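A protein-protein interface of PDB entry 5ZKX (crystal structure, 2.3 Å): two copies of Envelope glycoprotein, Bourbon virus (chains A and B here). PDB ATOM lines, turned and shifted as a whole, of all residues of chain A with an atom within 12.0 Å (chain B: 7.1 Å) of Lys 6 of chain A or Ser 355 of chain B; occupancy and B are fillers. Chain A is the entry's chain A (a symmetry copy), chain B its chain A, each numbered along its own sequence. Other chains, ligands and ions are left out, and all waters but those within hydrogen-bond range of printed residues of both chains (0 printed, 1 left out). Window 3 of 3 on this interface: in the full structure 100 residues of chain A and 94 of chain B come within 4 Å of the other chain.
N of Gly 11 of chain A lies close to SD of Met 353 of chain B (3.8 Å).
N of Gln 10 of chain A lies within hydrogen-bond range of O of Val 354 of chain B (3.0 Å).
OG of Ser 355 of chain B is in hydrogen-bond range of O of Gln 8 of chain A (2.8 Å).
OG of Ser 355 of chain B lies within hydrogen-bond range of OE1 of Gln 9 of chain A (2.8 Å).
The backbone NH (N) of Asn 5 of chain A sits at hydrogen-bond distance from the backbone carbonyl oxygen (O) of Pro 356 of chain B (3.2 Å).
The side-chain sulfur (SG) of Cys 357 of chain B is disulfide-bonded to the side-chain sulfur (SG) of Cys 4 of chain A (2.0 Å).
The backbone carbonyl oxygen of Gln 8 of chain A sits close to the backbone carbonyl oxygen of Val 354 of chain B (3.5 Å).
N of Pro 12 of chain A lies close to SD of Met 353 of chain B (3.4 Å).
O of Met 342 of chain B sits at hydrogen-bond distance from NE of Arg 332 of chain B.
The backbone carbonyl oxygen (O) of Ala 343 of chain B sits at hydrogen-bond distance from the backbone NH (N) of Ser 355 of chain B, at 2.9 Å.
N of Ala 343 of chain B sits at hydrogen-bond distance from SG of Cys 357 of chain B (3.8 Å).
The backbone carbonyl oxygen (O) of Lys 345 of chain B sits at hydrogen-bond distance from the backbone NH (N) of Met 353 of chain B (2.7 Å).
N of Gln 7 of chain A sits close to OD1 of Asn 5 of chain A, at 3.5 Å.
O of Lys 6 of chain A lies close to OE1 of Gln 9 of chain A (3.3 Å).
Among the printed residues, merely in contact across the chains: Gln 9 of chain A with Val 354 of chain B (3.1 Å), Gln 10 of chain A with Met 353 of chain B (3.3 Å), Asn 5 of chain A with Ser 355 of chain B (3.4 Å), Gln 9 of chain A with Met 353 of chain B (3.5 Å), Gln 8 of chain A with Pro 356 of chain B (3.7 Å), Cys 4 of chain A with Pro 356 of chain B (3.7 Å), Cys 4 of chain A with Ala 343 of chain B (3.8 Å), Cys 4 of chain A with Arg 332 of chain B (3.9 Å), Leu 3 of chain A with Cys 357 of chain B (3.9 Å) and Lys 6 of chain A with Ser 355 of chain B (3.998 Å).
Of the printed residues of chain B, Lys 6 of chain A touches Ser 355.
Printed residues of chain B within 4 Å of Gly 11 of chain A: Met 353.
Of the printed residues of chain B, Pro 12 of chain A touches Met 353 (3.4 Å).
Asp 331 of chain B touches none of the printed residues of chain A.
No residue of chain A comes within 4 Å of Met 342 of chain B.
No residue of chain A comes within 4 Å of Ser 344 of chain B.
No residue of chain A comes within 4 Å of Lys 345 of chain B.
Val 354 of chain B touches three residues of chain A.
Of the printed residues of chain A, Ser 355 of chain B touches Asn 5 (3.4 Å), Lys 6 (3.998 Å), Gln 8 (2.8 Å) and Gln 9 (2.8 Å).
Of the printed residues of chain A, Pro 356 of chain B touches Cys 4 (3.7 Å), Asn 5 (3.2 Å) and Gln 8 (3.7 Å).
Printed residues of chain A within 4 Å of Cys 357 of chain B: Leu 3 and Cys 4.
The nearest printed residue of chain B that does not touch Lys 6 of chain A is Pro 356 of chain B (5.5 Å).
Of the 11 printed residues of chain A, 9 touch a printed residue of chain B.
Hydrophobic or aromatic side chains of chain A that line the printed part of chain B: Pro 12.
Of the 12 printed residues of chain B, 7 touch a printed residue of chain A.
Among the printed residues, no Asp or Glu carboxylate lies within 4 Å of a Lys or Arg side-chain nitrogen of the other chain.
No position is printed for both chains.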
ATOM      1  N   LEU A   3      -7.596  -3.224 -34.516  1.00  0.00           N
ATOM      2  CA  LEU A   3      -7.808  -3.431 -33.090  1.00  0.00           C
ATOM      3  C   LEU A   3      -9.204  -2.982 -32.672  1.00  0.00           C
ATOM      4  O   LEU A   3      -9.825  -2.143 -33.325  1.00  0.00           O
ATOM      5  CB  LEU A   3      -6.750  -2.682 -32.272  1.00  0.00           C
ATOM      6  CG  LEU A   3      -6.558  -3.124 -30.816  1.00  0.00           C
ATOM      7  CD1 LEU A   3      -5.775  -4.426 -30.744  1.00  0.00           C
ATOM      8  CD2 LEU A   3      -5.872  -2.037 -30.009  1.00  0.00           C
ATOM      9  N   CYS A   4      -9.692  -3.558 -31.581  1.00  0.00           N
ATOM     10  CA  CYS A   4     -10.931  -3.149 -30.946  1.00  0.00           C
ATOM     11  C   CYS A   4     -10.620  -2.424 -29.645  1.00  0.00           C
ATOM     12  O   CYS A   4      -9.495  -2.446 -29.142  1.00  0.00           O
ATOM     13  CB  CYS A   4     -11.836  -4.356 -30.678  1.00  0.00           C
ATOM     14  SG  CYS A   4     -12.233  -5.335 -32.140  1.00  0.00           S
ATOM     15  N   ASN A   5     -11.641  -1.777 -29.101  1.00  0.00           N
ATOM     16  CA  ASN A   5     -11.546  -1.106 -27.812  1.00  0.00           C
ATOM     17  C   ASN A   5     -12.358  -1.937 -26.821  1.00  0.00           C
ATOM     18  O   ASN A   5     -13.512  -1.624 -26.524  1.00  0.00           O
ATOM     19  CB  ASN A   5     -12.052   0.336 -27.903  1.00  0.00           C
ATOM     20  CG  ASN A   5     -11.702   1.154 -26.679  1.00  0.00           C
ATOM     21  OD1 ASN A   5     -10.923   0.720 -25.834  1.00  0.00           O
ATOM     22  ND2 ASN A   5     -12.280   2.346 -26.578  1.00  0.00           N
ATOM     23  N   LYS A   6     -11.732  -2.990 -26.287  1.00  0.00           N
ATOM     24  CA  LYS A   6     -12.355  -3.856 -25.292  1.00  0.00           C
ATOM     25  C   LYS A   6     -12.718  -3.116 -24.021  1.00  0.00           C
ATOM     26  O   LYS A   6     -13.250  -3.717 -23.085  1.00  0.00           O
ATOM     27  CB  LYS A   6     -11.419  -5.016 -24.961  1.00  0.00           C
ATOM     28  CG  LYS A   6     -10.547  -5.443 -26.133  1.00  0.00           C
ATOM     29  CD  LYS A   6      -9.820  -6.754 -25.860  1.00  0.00           C
ATOM     30  CE  LYS A   6      -8.483  -6.798 -26.589  1.00  0.00           C
ATOM     31  NZ  LYS A   6      -7.431  -6.031 -25.863  1.00  0.00           N
ATOM     32  N   GLN A   7     -12.442  -1.818 -23.985  1.00  0.00           N
ATOM     33  CA  GLN A   7     -12.710  -0.995 -22.817  1.00  0.00           C
ATOM     34  C   GLN A   7     -14.201  -0.877 -22.562  1.00  0.00           C
ATOM     35  O   GLN A   7     -14.657  -1.031 -21.427  1.00  0.00           O
ATOM     36  CB  GLN A   7     -12.148   0.398 -23.022  1.00  0.00           C
ATOM     37  CG  GLN A   7     -11.686   1.103 -21.771  1.00  0.00           C
ATOM     38  CD  GLN A   7     -10.323   0.625 -21.296  1.00  0.00           C
ATOM     39  OE1 GLN A   7     -10.213  -0.264 -20.451  1.00  0.00           O
ATOM     40  NE2 GLN A   7      -9.270   1.224 -21.845  1.00  0.00           N
ATOM     41  N   GLN A   8     -14.975  -0.585 -23.602  1.00  0.00           N
ATOM     42  CA  GLN A   8     -16.324  -0.055 -23.454  1.00  0.00           C
ATOM     43  C   GLN A   8     -17.340  -1.011 -24.060  1.00  0.00           C
ATOM     44  O   GLN A   8     -17.274  -1.327 -25.255  1.00  0.00           O
ATOM     45  CB  GLN A   8     -16.403   1.321 -24.105  1.00  0.00           C
ATOM     46  CG  GLN A   8     -15.201   2.200 -23.787  1.00  0.00           C
ATOM     47  CD  GLN A   8     -15.065   2.549 -22.314  1.00  0.00           C
ATOM     48  OE1 GLN A   8     -15.938   2.242 -21.507  1.00  0.00           O
ATOM     49  NE2 GLN A   8     -13.999   3.257 -21.973  1.00  0.00           N
ATOM     50  N   GLN A   9     -18.281  -1.444 -23.241  1.00  0.00           N
ATOM     51  CA  GLN A   9     -19.251  -2.441 -23.636  1.00  0.00           C
ATOM     52  C   GLN A   9     -20.554  -1.765 -24.047  1.00  0.00           C
ATOM     53  O   GLN A   9     -20.663  -0.538 -24.109  1.00  0.00           O
ATOM     54  CB  GLN A   9     -19.470  -3.428 -22.494  1.00  0.00           C
ATOM     55  CG  GLN A   9     -18.228  -3.701 -21.670  1.00  0.00           C
ATOM     56  CD  GLN A   9     -17.188  -4.518 -22.411  1.00  0.00           C
ATOM     57  OE1 GLN A   9     -16.523  -4.035 -23.333  1.00  0.00           O
ATOM     58  NE2 GLN A   9     -17.044  -5.772 -22.011  1.00  0.00           N
ATOM     59  N   GLN A  10     -21.548  -2.590 -24.357  1.00  0.00           N
ATOM     60  CA  GLN A  10     -22.906  -2.106 -24.547  1.00  0.00           C
ATOM     61  C   GLN A  10     -23.842  -3.301 -24.499  1.00  0.00           C
ATOM     62  O   GLN A  10     -23.624  -4.292 -25.203  1.00  0.00           O
ATOM     63  CB  GLN A  10     -23.063  -1.356 -25.866  1.00  0.00           C
ATOM     64  CG  GLN A  10     -24.472  -0.865 -26.081  1.00  0.00           C
ATOM     65  CD  GLN A  10     -25.029  -0.126 -24.877  1.00  0.00           C
ATOM     66  OE1 GLN A  10     -25.834  -0.668 -24.117  1.00  0.00           O
ATOM     67  NE2 GLN A  10     -24.613   1.125 -24.705  1.00  0.00           N
ATOM     68  N   GLY A  11     -24.870  -3.207 -23.663  1.00  0.00           N
ATOM     69  CA  GLY A  11     -25.840  -4.264 -23.543  1.00  0.00           C
ATOM     70  C   GLY A  11     -26.395  -4.379 -22.139  1.00  0.00           C
ATOM     71  O   GLY A  11     -26.623  -3.377 -21.456  1.00  0.00           O
ATOM     72  N   PRO A  12     -26.632  -5.617 -21.676  1.00  0.00           N
ATOM     73  CA  PRO A  12     -26.413  -6.848 -22.443  1.00  0.00           C
ATOM     74  C   PRO A  12     -27.448  -7.046 -23.538  1.00  0.00           C
ATOM     75  O   PRO A  12     -28.555  -6.522 -23.443  1.00  0.00           O
ATOM     76  CB  PRO A  12     -26.528  -7.945 -21.385  1.00  0.00           C
ATOM     77  CG  PRO A  12     -27.429  -7.368 -20.353  1.00  0.00           C
ATOM     78  CD  PRO A  12     -27.127  -5.894 -20.318  1.00  0.00           C
ATOM     79  N   PHE A  13     -27.076  -7.782 -24.576  1.00  0.00           N
ATOM     80  CA  PHE A  13     -27.955  -8.034 -25.703  1.00  0.00           C
ATOM     81  C   PHE A  13     -28.442  -9.474 -25.673  1.00  0.00           C
ATOM     82  O   PHE A  13     -27.979 -10.303 -24.886  1.00  0.00           O
ATOM     83  CB  PHE A  13     -27.242  -7.740 -27.026  1.00  0.00           C
ATOM     84  CG  PHE A  13     -27.167  -6.280 -27.362  1.00  0.00           C
ATOM     85  CD1 PHE A  13     -28.286  -5.600 -27.811  1.00  0.00           C
ATOM     86  CD2 PHE A  13     -25.978  -5.585 -27.224  1.00  0.00           C
ATOM     87  CE1 PHE A  13     -28.217  -4.255 -28.120  1.00  0.00           C
ATOM     88  CE2 PHE A  13     -25.905  -4.239 -27.530  1.00  0.00           C
ATOM     89  CZ  PHE A  13     -27.027  -3.574 -27.978  1.00  0.00           C
ATOM     90  N   ASP B 331     -14.908 -13.643 -31.548  1.00  0.00           N
ATOM     91  CA  ASP B 331     -15.588 -12.460 -31.033  1.00  0.00           C
ATOM     92  C   ASP B 331     -15.865 -11.414 -32.105  1.00  0.00           C
ATOM     93  O   ASP B 331     -16.513 -10.407 -31.806  1.00  0.00           O
ATOM     94  CB  ASP B 331     -14.769 -11.834 -29.901  1.00  0.00           C
ATOM     95  CG  ASP B 331     -13.388 -11.388 -30.350  1.00  0.00           C
ATOM     96  OD1 ASP B 331     -12.977 -11.739 -31.476  1.00  0.00           O
ATOM     97  OD2 ASP B 331     -12.710 -10.687 -29.571  1.00  0.00           O
ATOM     98  N   ARG B 332     -15.393 -11.616 -33.333  1.00  0.00           N
ATOM     99  CA  ARG B 332     -15.669 -10.694 -34.426  1.00  0.00           C
ATOM    100  C   ARG B 332     -16.790 -11.175 -35.337  1.00  0.00           C
ATOM    101  O   ARG B 332     -17.155 -10.462 -36.277  1.00  0.00           O
ATOM    102  CB  ARG B 332     -14.403 -10.460 -35.253  1.00  0.00           C
ATOM    103  CG  ARG B 332     -13.263  -9.838 -34.472  1.00  0.00           C
ATOM    104  CD  ARG B 332     -13.641  -8.468 -33.941  1.00  0.00           C
ATOM    105  NE  ARG B 332     -14.157  -7.604 -34.997  1.00  0.00           N
ATOM    106  CZ  ARG B 332     -13.395  -6.925 -35.848  1.00  0.00           C
ATOM    107  NH1 ARG B 332     -12.075  -7.002 -35.770  1.00  0.00           N
ATOM    108  NH2 ARG B 332     -13.955  -6.165 -36.779  1.00  0.00           N
ATOM    109  N   PRO B 341     -18.257  -3.170 -37.799  1.00  0.00           N
ATOM    110  CA  PRO B 341     -17.069  -3.627 -37.066  1.00  0.00           C
ATOM    111  C   PRO B 341     -17.260  -3.577 -35.557  1.00  0.00           C
ATOM    112  O   PRO B 341     -17.383  -2.497 -34.973  1.00  0.00           O
ATOM    113  CB  PRO B 341     -15.974  -2.657 -37.529  1.00  0.00           C
ATOM    114  CG  PRO B 341     -16.709  -1.434 -37.963  1.00  0.00           C
ATOM    115  CD  PRO B 341     -18.022  -1.907 -38.519  1.00  0.00           C
ATOM    116  N   MET B 342     -17.294  -4.745 -34.919  1.00  0.00           N
ATOM    117  CA  MET B 342     -17.469  -4.812 -33.475  1.00  0.00           C
ATOM    118  C   MET B 342     -16.923  -6.137 -32.967  1.00  0.00           C
ATOM    119  O   MET B 342     -16.721  -7.083 -33.734  1.00  0.00           O
ATOM    120  CB  MET B 342     -18.941  -4.654 -33.077  1.00  0.00           C
ATOM    121  CG  MET B 342     -19.764  -5.915 -33.263  1.00  0.00           C
ATOM    122  SD  MET B 342     -21.474  -5.784 -32.695  1.00  0.00           S
ATOM    123  CE  MET B 342     -21.874  -4.089 -33.111  1.00  0.00           C
ATOM    124  N   ALA B 343     -16.685  -6.187 -31.659  1.00  0.00           N
ATOM    125  CA  ALA B 343     -16.293  -7.403 -30.968  1.00  0.00           C
ATOM    126  C   ALA B 343     -17.317  -7.729 -29.891  1.00  0.00           C
ATOM    127  O   ALA B 343     -17.887  -6.831 -29.264  1.00  0.00           O
ATOM    128  CB  ALA B 343     -14.903  -7.277 -30.335  1.00  0.00           C
ATOM    129  N   SER B 344     -17.544  -9.022 -29.679  1.00  0.00           N
ATOM    130  CA  SER B 344     -18.534  -9.501 -28.728  1.00  0.00           C
ATOM    131  C   SER B 344     -17.854 -10.098 -27.501  1.00  0.00           C
ATOM    132  O   SER B 344     -16.722 -10.582 -27.572  1.00  0.00           O
ATOM    133  CB  SER B 344     -19.448 -10.552 -29.366  1.00  0.00           C
ATOM    134  OG  SER B 344     -18.801 -11.809 -29.442  1.00  0.00           O
ATOM    135  N   LYS B 345     -18.566 -10.058 -26.375  1.00  0.00           N
ATOM    136  CA  LYS B 345     -18.095 -10.658 -25.128  1.00  0.00           C
ATOM    137  C   LYS B 345     -19.323 -11.060 -24.324  1.00  0.00           C
ATOM    138  O   LYS B 345     -20.097 -10.196 -23.902  1.00  0.00           O
ATOM    139  CB  LYS B 345     -17.210  -9.692 -24.341  1.00  0.00           C
ATOM    140  CG  LYS B 345     -16.555 -10.304 -23.106  1.00  0.00           C
ATOM    141  CD  LYS B 345     -15.292  -9.548 -22.710  1.00  0.00           C
ATOM    142  CE  LYS B 345     -14.654 -10.141 -21.461  1.00  0.00           C
ATOM    143  NZ  LYS B 345     -14.403 -11.603 -21.594  1.00  0.00           N
ATOM    144  N   MET B 353     -22.110  -8.487 -24.425  1.00  0.00           N
ATOM    145  CA  MET B 353     -21.873  -7.065 -24.612  1.00  0.00           C
ATOM    146  C   MET B 353     -21.089  -6.838 -25.898  1.00  0.00           C
ATOM    147  O   MET B 353     -20.499  -7.760 -26.466  1.00  0.00           O
ATOM    148  CB  MET B 353     -21.109  -6.461 -23.429  1.00  0.00           C
ATOM    149  CG  MET B 353     -21.671  -6.814 -22.072  1.00  0.00           C
ATOM    150  SD  MET B 353     -23.209  -5.961 -21.699  1.00  0.00           S
ATOM    151  CE  MET B 353     -22.640  -4.304 -21.358  1.00  0.00           C
ATOM    152  N   VAL B 354     -21.074  -5.586 -26.342  1.00  0.00           N
ATOM    153  CA  VAL B 354     -20.545  -5.223 -27.648  1.00  0.00           C
ATOM    154  C   VAL B 354     -19.559  -4.074 -27.486  1.00  0.00           C
ATOM    155  O   VAL B 354     -19.853  -3.088 -26.800  1.00  0.00           O
ATOM    156  CB  VAL B 354     -21.678  -4.839 -28.618  1.00  0.00           C
ATOM    157  CG1 VAL B 354     -21.179  -3.871 -29.675  1.00  0.00           C
ATOM    158  CG2 VAL B 354     -22.271  -6.091 -29.250  1.00  0.00           C
ATOM    159  N   SER B 355     -18.393  -4.202 -28.119  1.00  0.00           N
ATOM    160  CA  SER B 355     -17.370  -3.172 -28.125  1.00  0.00           C
ATOM    161  C   SER B 355     -17.071  -2.738 -29.555  1.00  0.00           C
ATOM    162  O   SER B 355     -17.111  -3.558 -30.475  1.00  0.00           O
ATOM    163  CB  SER B 355     -16.080  -3.668 -27.457  1.00  0.00           C
ATOM    164  OG  SER B 355     -16.277  -3.866 -26.068  1.00  0.00           O
ATOM    165  N   PRO B 356     -16.769  -1.460 -29.774  1.00  0.00           N
ATOM    166  CA  PRO B 356     -16.578  -0.968 -31.140  1.00  0.00           C
ATOM    167  C   PRO B 356     -15.213  -1.318 -31.707  1.00  0.00           C
ATOM    168  O   PRO B 356     -14.224  -1.455 -30.984  1.00  0.00           O
ATOM    169  CB  PRO B 356     -16.728   0.549 -30.986  1.00  0.00           C
ATOM    170  CG  PRO B 356     -16.249   0.813 -29.598  1.00  0.00           C
ATOM    171  CD  PRO B 356     -16.679  -0.379 -28.777  1.00  0.00           C
ATOM    172  N   CYS B 357     -15.176  -1.459 -33.030  1.00  0.00           N
ATOM    173  CA  CYS B 357     -13.942  -1.745 -33.754  1.00  0.00           C
ATOM    174  C   CYS B 357     -13.690  -0.696 -34.832  1.00  0.00           C
ATOM    175  O   CYS B 357     -12.697  -0.761 -35.557  1.00  0.00           O
ATOM    176  CB  CYS B 357     -13.994  -3.137 -34.386  1.00  0.00           C
ATOM    177  SG  CYS B 357     -13.730  -4.488 -33.227  1.00  0.00           S
